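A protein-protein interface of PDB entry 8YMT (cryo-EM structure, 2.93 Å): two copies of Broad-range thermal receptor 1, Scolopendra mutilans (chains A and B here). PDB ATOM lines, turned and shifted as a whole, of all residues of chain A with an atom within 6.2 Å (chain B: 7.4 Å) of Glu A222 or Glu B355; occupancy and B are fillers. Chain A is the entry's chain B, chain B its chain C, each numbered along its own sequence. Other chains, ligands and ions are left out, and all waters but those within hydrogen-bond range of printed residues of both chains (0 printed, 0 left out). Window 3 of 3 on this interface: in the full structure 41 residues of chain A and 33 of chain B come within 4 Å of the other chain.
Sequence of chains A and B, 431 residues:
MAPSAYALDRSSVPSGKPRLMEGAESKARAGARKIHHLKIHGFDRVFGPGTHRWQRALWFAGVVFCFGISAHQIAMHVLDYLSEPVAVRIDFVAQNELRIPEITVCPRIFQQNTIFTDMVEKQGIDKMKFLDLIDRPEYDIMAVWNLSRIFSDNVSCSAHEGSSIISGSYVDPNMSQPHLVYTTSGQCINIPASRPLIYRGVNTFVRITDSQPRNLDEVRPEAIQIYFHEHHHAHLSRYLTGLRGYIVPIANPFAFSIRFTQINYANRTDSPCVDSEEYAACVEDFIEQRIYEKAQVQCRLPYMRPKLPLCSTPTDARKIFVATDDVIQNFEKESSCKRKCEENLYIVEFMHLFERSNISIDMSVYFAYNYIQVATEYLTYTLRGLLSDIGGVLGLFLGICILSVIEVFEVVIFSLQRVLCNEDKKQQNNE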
ATOM      1  N   ARG A 108     -14.400  -7.721 -25.488  1.00  0.00           N
ATOM      2  CA  ARG A 108     -13.254  -8.194 -26.244  1.00  0.00           C
ATOM      3  C   ARG A 108     -12.411  -6.999 -26.679  1.00  0.00           C
ATOM      4  O   ARG A 108     -12.783  -5.842 -26.480  1.00  0.00           O
ATOM      5  CB  ARG A 108     -13.699  -9.003 -27.459  1.00  0.00           C
ATOM      6  CG  ARG A 108     -14.229 -10.396 -27.143  1.00  0.00           C
ATOM      7  CD  ARG A 108     -14.826 -11.025 -28.387  1.00  0.00           C
ATOM      8  NE  ARG A 108     -15.217 -12.416 -28.207  1.00  0.00           N
ATOM      9  CZ  ARG A 108     -15.856 -13.131 -29.121  1.00  0.00           C
ATOM     10  NH1 ARG A 108     -16.239 -12.597 -30.269  1.00  0.00           N
ATOM     11  NH2 ARG A 108     -16.111 -14.413 -28.879  1.00  0.00           N
ATOM     12  N   GLN A 112     -12.456  -7.449 -31.653  1.00  0.00           N
ATOM     13  CA  GLN A 112     -13.283  -8.630 -31.446  1.00  0.00           C
ATOM     14  C   GLN A 112     -14.591  -8.300 -30.740  1.00  0.00           C
ATOM     15  O   GLN A 112     -15.449  -9.180 -30.604  1.00  0.00           O
ATOM     16  CB  GLN A 112     -12.511  -9.685 -30.652  1.00  0.00           C
ATOM     17  CG  GLN A 112     -11.286 -10.225 -31.363  1.00  0.00           C
ATOM     18  CD  GLN A 112     -10.552 -11.260 -30.542  1.00  0.00           C
ATOM     19  OE1 GLN A 112     -10.940 -11.563 -29.415  1.00  0.00           O
ATOM     20  NE2 GLN A 112      -9.483 -11.808 -31.103  1.00  0.00           N
ATOM     21  N   THR A 114     -17.889  -7.324 -30.972  1.00  0.00           N
ATOM     22  CA  THR A 114     -18.827  -7.257 -32.093  1.00  0.00           C
ATOM     23  C   THR A 114     -20.064  -6.460 -31.680  1.00  0.00           C
ATOM     24  O   THR A 114     -21.210  -6.886 -31.846  1.00  0.00           O
ATOM     25  CB  THR A 114     -19.202  -8.657 -32.562  1.00  0.00           C
ATOM     26  OG1 THR A 114     -20.037  -9.288 -31.583  1.00  0.00           O
ATOM     27  CG2 THR A 114     -17.952  -9.500 -32.783  1.00  0.00           C
ATOM     28  N   VAL A 219     -26.500  -6.208 -32.723  1.00  0.00           N
ATOM     29  CA  VAL A 219     -25.764  -7.427 -32.412  1.00  0.00           C
ATOM     30  C   VAL A 219     -25.300  -7.349 -30.965  1.00  0.00           C
ATOM     31  O   VAL A 219     -24.876  -6.288 -30.491  1.00  0.00           O
ATOM     32  CB  VAL A 219     -24.582  -7.612 -33.376  1.00  0.00           C
ATOM     33  CG1 VAL A 219     -23.765  -8.835 -32.985  1.00  0.00           C
ATOM     34  CG2 VAL A 219     -25.074  -7.742 -34.815  1.00  0.00           C
ATOM     35  N   ARG A 220     -25.403  -8.466 -30.250  1.00  0.00           N
ATOM     36  CA  ARG A 220     -25.079  -8.480 -28.833  1.00  0.00           C
ATOM     37  C   ARG A 220     -23.677  -9.024 -28.576  1.00  0.00           C
ATOM     38  O   ARG A 220     -23.154  -9.826 -29.353  1.00  0.00           O
ATOM     39  CB  ARG A 220     -26.112  -9.304 -28.068  1.00  0.00           C
ATOM     40  CG  ARG A 220     -27.506  -8.705 -28.105  1.00  0.00           C
ATOM     41  CD  ARG A 220     -27.521  -7.421 -27.279  1.00  0.00           C
ATOM     42  NE  ARG A 220     -28.841  -6.817 -27.159  1.00  0.00           N
ATOM     43  CZ  ARG A 220     -29.325  -5.904 -27.990  1.00  0.00           C
ATOM     44  NH1 ARG A 220     -28.618  -5.456 -29.016  1.00  0.00           N
ATOM     45  NH2 ARG A 220     -30.545  -5.418 -27.781  1.00  0.00           N
ATOM     46  N   PRO A 221     -23.049  -8.591 -27.484  1.00  0.00           N
ATOM     47  CA  PRO A 221     -21.715  -9.103 -27.154  1.00  0.00           C
ATOM     48  C   PRO A 221     -21.752 -10.587 -26.835  1.00  0.00           C
ATOM     49  O   PRO A 221     -22.686 -11.087 -26.206  1.00  0.00           O
ATOM     50  CB  PRO A 221     -21.308  -8.271 -25.932  1.00  0.00           C
ATOM     51  CG  PRO A 221     -22.595  -7.844 -25.320  1.00  0.00           C
ATOM     52  CD  PRO A 221     -23.562  -7.677 -26.448  1.00  0.00           C
ATOM     53  N   GLU A 222     -20.715 -11.294 -27.282  1.00  0.00           N
ATOM     54  CA  GLU A 222     -20.613 -12.732 -27.077  1.00  0.00           C
ATOM     55  C   GLU A 222     -19.716 -13.086 -25.899  1.00  0.00           C
ATOM     56  O   GLU A 222     -19.947 -14.098 -25.229  1.00  0.00           O
ATOM     57  CB  GLU A 222     -20.077 -13.404 -28.344  1.00  0.00           C
ATOM     58  CG  GLU A 222     -20.926 -13.164 -29.582  1.00  0.00           C
ATOM     59  CD  GLU A 222     -20.092 -12.927 -30.827  1.00  0.00           C
ATOM     60  OE1 GLU A 222     -20.558 -12.194 -31.723  1.00  0.00           O
ATOM     61  OE2 GLU A 222     -18.973 -13.476 -30.910  1.00  0.00           O
ATOM     62  N   ALA A 223     -18.703 -12.268 -25.629  1.00  0.00           N
ATOM     63  CA  ALA A 223     -17.687 -12.585 -24.638  1.00  0.00           C
ATOM     64  C   ALA A 223     -17.462 -11.379 -23.742  1.00  0.00           C
ATOM     65  O   ALA A 223     -17.892 -10.262 -24.043  1.00  0.00           O
ATOM     66  CB  ALA A 223     -16.363 -12.982 -25.298  1.00  0.00           C
ATOM     67  N   ILE A 224     -16.774 -11.617 -22.625  1.00  0.00           N
ATOM     68  CA  ILE A 224     -16.262 -10.545 -21.786  1.00  0.00           C
ATOM     69  C   ILE A 224     -14.931 -10.980 -21.194  1.00  0.00           C
ATOM     70  O   ILE A 224     -14.638 -12.170 -21.044  1.00  0.00           O
ATOM     71  CB  ILE A 224     -17.235 -10.132 -20.660  1.00  0.00           C
ATOM     72  CG1 ILE A 224     -17.683 -11.351 -19.861  1.00  0.00           C
ATOM     73  CG2 ILE A 224     -18.433  -9.402 -21.238  1.00  0.00           C
ATOM     74  CD1 ILE A 224     -18.442 -10.990 -18.621  1.00  0.00           C
ATOM     75  N   ILE A 247     -11.446 -14.781 -20.897  1.00  0.00           N
ATOM     76  CA  ILE A 247     -12.474 -14.504 -21.895  1.00  0.00           C
ATOM     77  C   ILE A 247     -13.571 -15.543 -21.694  1.00  0.00           C
ATOM     78  O   ILE A 247     -13.394 -16.717 -22.014  1.00  0.00           O
ATOM     79  CB  ILE A 247     -11.917 -14.544 -23.317  1.00  0.00           C
ATOM     80  CG1 ILE A 247     -10.752 -13.570 -23.460  1.00  0.00           C
ATOM     81  CG2 ILE A 247     -13.015 -14.206 -24.319  1.00  0.00           C
ATOM     82  CD1 ILE A 247     -10.112 -13.573 -24.827  1.00  0.00           C
ATOM     83  N   VAL A 248     -14.713 -15.110 -21.179  1.00  0.00           N
ATOM     84  CA  VAL A 248     -15.794 -16.036 -20.847  1.00  0.00           C
ATOM     85  C   VAL A 248     -17.066 -15.542 -21.517  1.00  0.00           C
ATOM     86  O   VAL A 248     -17.264 -14.329 -21.697  1.00  0.00           O
ATOM     87  CB  VAL A 248     -15.978 -16.182 -19.319  1.00  0.00           C
ATOM     88  CG1 VAL A 248     -14.721 -16.755 -18.690  1.00  0.00           C
ATOM     89  CG2 VAL A 248     -16.335 -14.847 -18.691  1.00  0.00           C
ATOM     90  N   PRO A 249     -17.959 -16.456 -21.898  1.00  0.00           N
ATOM     91  CA  PRO A 249     -19.239 -16.036 -22.473  1.00  0.00           C
ATOM     92  C   PRO A 249     -20.299 -15.482 -21.534  1.00  0.00           C
ATOM     93  O   PRO A 249     -20.285 -15.720 -20.324  1.00  0.00           O
ATOM     94  CB  PRO A 249     -19.707 -17.254 -23.280  1.00  0.00           C
ATOM     95  CG  PRO A 249     -18.892 -18.420 -22.773  1.00  0.00           C
ATOM     96  CD  PRO A 249     -17.867 -17.922 -21.790  1.00  0.00           C
ATOM     97  N   ILE A 250     -21.231 -14.735 -22.115  1.00  0.00           N
ATOM     98  CA  ILE A 250     -22.322 -14.128 -21.371  1.00  0.00           C
ATOM     99  C   ILE A 250     -23.680 -14.592 -21.894  1.00  0.00           C
ATOM    100  O   ILE A 250     -24.708 -14.020 -21.551  1.00  0.00           O
ATOM    101  CB  ILE A 250     -22.209 -12.593 -21.387  1.00  0.00           C
ATOM    102  CG1 ILE A 250     -22.244 -12.075 -22.823  1.00  0.00           C
ATOM    103  CG2 ILE A 250     -20.927 -12.164 -20.714  1.00  0.00           C
ATOM    104  CD1 ILE A 250     -22.270 -10.576 -22.925  1.00  0.00           C
ATOM    105  N   ALA A 251     -23.691 -15.634 -22.729  1.00  0.00           N
ATOM    106  CA  ALA A 251     -24.954 -16.187 -23.198  1.00  0.00           C
ATOM    107  C   ALA A 251     -25.766 -16.734 -22.032  1.00  0.00           C
ATOM    108  O   ALA A 251     -26.988 -16.558 -21.973  1.00  0.00           O
ATOM    109  CB  ALA A 251     -24.694 -17.278 -24.235  1.00  0.00           C
ATOM    110  N   ARG B 207      -4.543 -25.449 -28.403  1.00  0.00           N
ATOM    111  CA  ARG B 207      -5.841 -25.754 -28.996  1.00  0.00           C
ATOM    112  C   ARG B 207      -5.653 -26.881 -30.005  1.00  0.00           C
ATOM    113  O   ARG B 207      -5.069 -26.680 -31.073  1.00  0.00           O
ATOM    114  CB  ARG B 207      -6.438 -24.498 -29.628  1.00  0.00           C
ATOM    115  CG  ARG B 207      -7.826 -24.659 -30.220  1.00  0.00           C
ATOM    116  CD  ARG B 207      -8.323 -23.324 -30.755  1.00  0.00           C
ATOM    117  NE  ARG B 207      -9.669 -23.399 -31.309  1.00  0.00           N
ATOM    118  CZ  ARG B 207      -9.951 -23.676 -32.575  1.00  0.00           C
ATOM    119  NH1 ARG B 207      -8.996 -23.833 -33.480  1.00  0.00           N
ATOM    120  NH2 ARG B 207     -11.222 -23.776 -32.951  1.00  0.00           N
ATOM    121  N   PRO B 253     -17.254 -27.568 -28.026  1.00  0.00           N
ATOM    122  CA  PRO B 253     -15.806 -27.336 -27.950  1.00  0.00           C
ATOM    123  C   PRO B 253     -15.319 -27.091 -26.531  1.00  0.00           C
ATOM    124  O   PRO B 253     -15.120 -25.946 -26.110  1.00  0.00           O
ATOM    125  CB  PRO B 253     -15.605 -26.108 -28.845  1.00  0.00           C
ATOM    126  CG  PRO B 253     -16.908 -25.425 -28.834  1.00  0.00           C
ATOM    127  CD  PRO B 253     -17.936 -26.501 -28.773  1.00  0.00           C
ATOM    128  N   PHE B 254     -15.123 -28.178 -25.790  1.00  0.00           N
ATOM    129  CA  PHE B 254     -14.626 -28.133 -24.418  1.00  0.00           C
ATOM    130  C   PHE B 254     -13.273 -27.488 -24.137  1.00  0.00           C
ATOM    131  O   PHE B 254     -12.526 -27.168 -25.068  1.00  0.00           O
ATOM    132  CB  PHE B 254     -14.738 -29.513 -23.753  1.00  0.00           C
ATOM    133  CG  PHE B 254     -13.864 -30.558 -24.382  1.00  0.00           C
ATOM    134  CD1 PHE B 254     -14.222 -31.153 -25.579  1.00  0.00           C
ATOM    135  CD2 PHE B 254     -12.671 -30.927 -23.792  1.00  0.00           C
ATOM    136  CE1 PHE B 254     -13.419 -32.101 -26.164  1.00  0.00           C
ATOM    137  CE2 PHE B 254     -11.867 -31.876 -24.377  1.00  0.00           C
ATOM    138  CZ  PHE B 254     -12.243 -32.463 -25.560  1.00  0.00           C
ATOM    139  N   HIS B 352     -14.930 -22.777 -18.733  1.00  0.00           N
ATOM    140  CA  HIS B 352     -15.903 -22.598 -19.815  1.00  0.00           C
ATOM    141  C   HIS B 352     -15.309 -21.804 -20.978  1.00  0.00           C
ATOM    142  O   HIS B 352     -15.138 -22.330 -22.081  1.00  0.00           O
ATOM    143  CB  HIS B 352     -17.162 -21.920 -19.265  1.00  0.00           C
ATOM    144  CG  HIS B 352     -18.389 -22.181 -20.081  1.00  0.00           C
ATOM    145  ND1 HIS B 352     -19.595 -21.557 -19.846  1.00  0.00           N
ATOM    146  CD2 HIS B 352     -18.591 -23.001 -21.138  1.00  0.00           C
ATOM    147  CE1 HIS B 352     -20.487 -21.980 -20.723  1.00  0.00           C
ATOM    148  NE2 HIS B 352     -19.903 -22.860 -21.518  1.00  0.00           N
ATOM    149  N   LEU B 353     -15.010 -20.525 -20.752  1.00  0.00           N
ATOM    150  CA  LEU B 353     -14.112 -19.751 -21.606  1.00  0.00           C
ATOM    151  C   LEU B 353     -14.541 -19.603 -23.062  1.00  0.00           C
ATOM    152  O   LEU B 353     -15.434 -20.309 -23.544  1.00  0.00           O
ATOM    153  CB  LEU B 353     -12.715 -20.351 -21.572  1.00  0.00           C
ATOM    154  CG  LEU B 353     -11.934 -19.866 -20.354  1.00  0.00           C
ATOM    155  CD1 LEU B 353     -11.713 -18.369 -20.429  1.00  0.00           C
ATOM    156  CD2 LEU B 353     -12.673 -20.214 -19.084  1.00  0.00           C
ATOM    157  N   PHE B 354     -13.864 -18.680 -23.757  1.00  0.00           N
ATOM    158  CA  PHE B 354     -14.105 -18.308 -25.148  1.00  0.00           C
ATOM    159  C   PHE B 354     -15.525 -18.658 -25.584  1.00  0.00           C
ATOM    160  O   PHE B 354     -16.486 -18.345 -24.872  1.00  0.00           O
ATOM    161  CB  PHE B 354     -13.077 -18.984 -26.069  1.00  0.00           C
ATOM    162  CG  PHE B 354     -11.645 -18.542 -25.856  1.00  0.00           C
ATOM    163  CD1 PHE B 354     -11.289 -17.668 -24.842  1.00  0.00           C
ATOM    164  CD2 PHE B 354     -10.652 -18.998 -26.705  1.00  0.00           C
ATOM    165  CE1 PHE B 354      -9.972 -17.273 -24.671  1.00  0.00           C
ATOM    166  CE2 PHE B 354      -9.338 -18.602 -26.542  1.00  0.00           C
ATOM    167  CZ  PHE B 354      -8.999 -17.739 -25.523  1.00  0.00           C
ATOM    168  N   GLU B 355     -15.675 -19.300 -26.742  1.00  0.00           N
ATOM    169  CA  GLU B 355     -16.983 -19.658 -27.280  1.00  0.00           C
ATOM    170  C   GLU B 355     -16.829 -20.829 -28.241  1.00  0.00           C
ATOM    171  O   GLU B 355     -15.793 -21.501 -28.244  1.00  0.00           O
ATOM    172  CB  GLU B 355     -17.659 -18.464 -27.972  1.00  0.00           C
ATOM    173  CG  GLU B 355     -18.130 -17.363 -27.029  1.00  0.00           C
ATOM    174  CD  GLU B 355     -17.064 -16.350 -26.687  1.00  0.00           C
ATOM    175  OE1 GLU B 355     -15.970 -16.389 -27.286  1.00  0.00           O
ATOM    176  OE2 GLU B 355     -17.320 -15.530 -25.785  1.00  0.00           O
ATOM    177  N   ARG B 356     -17.848 -21.081 -29.060  1.00  0.00           N
ATOM    178  CA  ARG B 356     -17.906 -22.299 -29.847  1.00  0.00           C
ATOM    179  C   ARG B 356     -17.530 -22.003 -31.291  1.00  0.00           C
ATOM    180  O   ARG B 356     -17.555 -20.858 -31.748  1.00  0.00           O
ATOM    181  CB  ARG B 356     -19.295 -22.937 -29.764  1.00  0.00           C
ATOM    182  CG  ARG B 356     -20.411 -22.035 -30.260  1.00  0.00           C
ATOM    183  CD  ARG B 356     -21.759 -22.724 -30.174  1.00  0.00           C
ATOM    184  NE  ARG B 356     -21.858 -23.845 -31.101  1.00  0.00           N
ATOM    185  CZ  ARG B 356     -22.099 -23.726 -32.400  1.00  0.00           C
ATOM    186  NH1 ARG B 356     -22.266 -22.542 -32.967  1.00  0.00           N
ATOM    187  NH2 ARG B 356     -22.175 -24.823 -33.147  1.00  0.00           N
ATOM    188  N   SER B 357     -17.171 -23.070 -32.004  1.00  0.00           N
ATOM    189  CA  SER B 357     -16.862 -23.006 -33.423  1.00  0.00           C
ATOM    190  C   SER B 357     -17.279 -24.326 -34.052  1.00  0.00           C
ATOM    191  O   SER B 357     -17.156 -25.383 -33.427  1.00  0.00           O
ATOM    192  CB  SER B 357     -15.370 -22.753 -33.666  1.00  0.00           C
ATOM    193  OG  SER B 357     -14.590 -23.858 -33.246  1.00  0.00           O
ATOM    194  N   ASP B 362     -12.818 -30.021 -30.787  1.00  0.00           N
ATOM    195  CA  ASP B 362     -12.068 -28.853 -30.345  1.00  0.00           C
ATOM    196  C   ASP B 362     -11.760 -29.018 -28.865  1.00  0.00           C
ATOM    197  O   ASP B 362     -12.680 -29.186 -28.058  1.00  0.00           O
ATOM    198  CB  ASP B 362     -12.861 -27.568 -30.581  1.00  0.00           C
ATOM    199  CG  ASP B 362     -11.973 -26.356 -30.765  1.00  0.00           C
ATOM    200  OD1 ASP B 362     -10.838 -26.362 -30.247  1.00  0.00           O
ATOM    201  OD2 ASP B 362     -12.416 -25.392 -31.423  1.00  0.00           O
ATOM    202  N   SER B 364      -9.299 -27.093 -26.074  1.00  0.00           N
ATOM    203  CA  SER B 364      -8.312 -26.115 -25.641  1.00  0.00           C
ATOM    204  C   SER B 364      -7.827 -26.461 -24.241  1.00  0.00           C
ATOM    205  O   SER B 364      -8.612 -26.488 -23.292  1.00  0.00           O
ATOM    206  CB  SER B 364      -8.912 -24.711 -25.658  1.00  0.00           C
ATOM    207  OG  SER B 364      -9.445 -24.397 -26.930  1.00  0.00           O
ATOM    208  N   TYR B 366      -5.695 -25.223 -21.256  1.00  0.00           N
ATOM    209  CA  TYR B 366      -5.211 -23.959 -20.726  1.00  0.00           C
ATOM    210  C   TYR B 366      -4.231 -24.216 -19.594  1.00  0.00           C
ATOM    211  O   TYR B 366      -4.375 -25.185 -18.839  1.00  0.00           O
ATOM    212  CB  TYR B 366      -6.369 -23.105 -20.210  1.00  0.00           C
ATOM    213  CG  TYR B 366      -7.155 -22.401 -21.287  1.00  0.00           C
ATOM    214  CD1 TYR B 366      -8.183 -23.045 -21.954  1.00  0.00           C
ATOM    215  CD2 TYR B 366      -6.883 -21.083 -21.623  1.00  0.00           C
ATOM    216  CE1 TYR B 366      -8.906 -22.407 -22.934  1.00  0.00           C
ATOM    217  CE2 TYR B 366      -7.602 -20.437 -22.601  1.00  0.00           C
ATOM    218  CZ  TYR B 366      -8.613 -21.103 -23.253  1.00  0.00           C
ATOM    219  OH  TYR B 366      -9.337 -20.465 -24.230  1.00  0.00           O
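O of Glu A222 lies close to OE2 of Glu B355, 3.0 Å away.
The backbone NH (N) of Phe B354 is in hydrogen-bond range of the backbone carbonyl oxygen (O) of Ile A247, at 2.7 Å.
The guanidinium group (NH2) of Arg A108 is in salt-bridge range of the side-chain carboxylate (OE1) of Glu B355, at 2.5 Å.
The side-chain hydroxyl of Thr A114 is in hydrogen-bond range of the side-chain carboxylate of Glu A222 (3.0 Å).
O of Glu A222 sits at hydrogen-bond distance from N of Ile A250, 3.4 Å away.
The guanidinium group of Arg A108 lies within salt-bridge range of the side-chain carboxylate of Glu A222, 2.9 Å away.
The backbone carbonyl oxygen (O) of Val A248 sits at hydrogen-bond distance from the backbone NH (N) of Ile A224 (2.9 Å).
Ala A223 touches Glu B355 (CB to OE2, 2.8 Å).
Ile A247 touches Leu B353 (O to CD1, 2.8 Å).
Leu B353 touches Val A248 (CD1 to CG1, 3.8 Å).
Leu B353 touches Pro A249.
O of Phe B354 touches CG of Pro A249, at 3.2 Å.
Pro A249 touches Glu B355 (CA to OE2, 3.9 Å).
Of chain B, only Glu B355 comes within 4 Å of Glu A222.
Printed residues of chain B within 4 Å of Ala A223: Glu B355.
Printed residues of chain A within 4 Å of Leu B353: Ile A247 (2.8 Å), Val A248 (3.8 Å) and Pro A249 (3.8 Å).
The nearest residue of chain B that does not touch Glu A222 is Phe B354 (5.5 Å).
The nearest residue of chain A that does not touch Glu B355 is Val A248 (4.3 Å).
The nearest printed residue of chain B that does not touch Pro A249 is His B352 (4.3 Å).
Printed residues of chain B that touch a printed residue of chain A: Leu B353, Phe B354 and Glu B355.
Hydrophobic or aromatic side chains of chain A within 4 Å of the printed part of chain B: Ala A223, Ile A247, Val A248 and Pro A249.
Among the printed residues, 9 pairs touch across the chains.
Among the printed residues, Asp or Glu carboxylates within 4 Å of a Lys or Arg side-chain nitrogen of the other chain: Arg A108 with Glu B355.
No position is printed for both chains.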
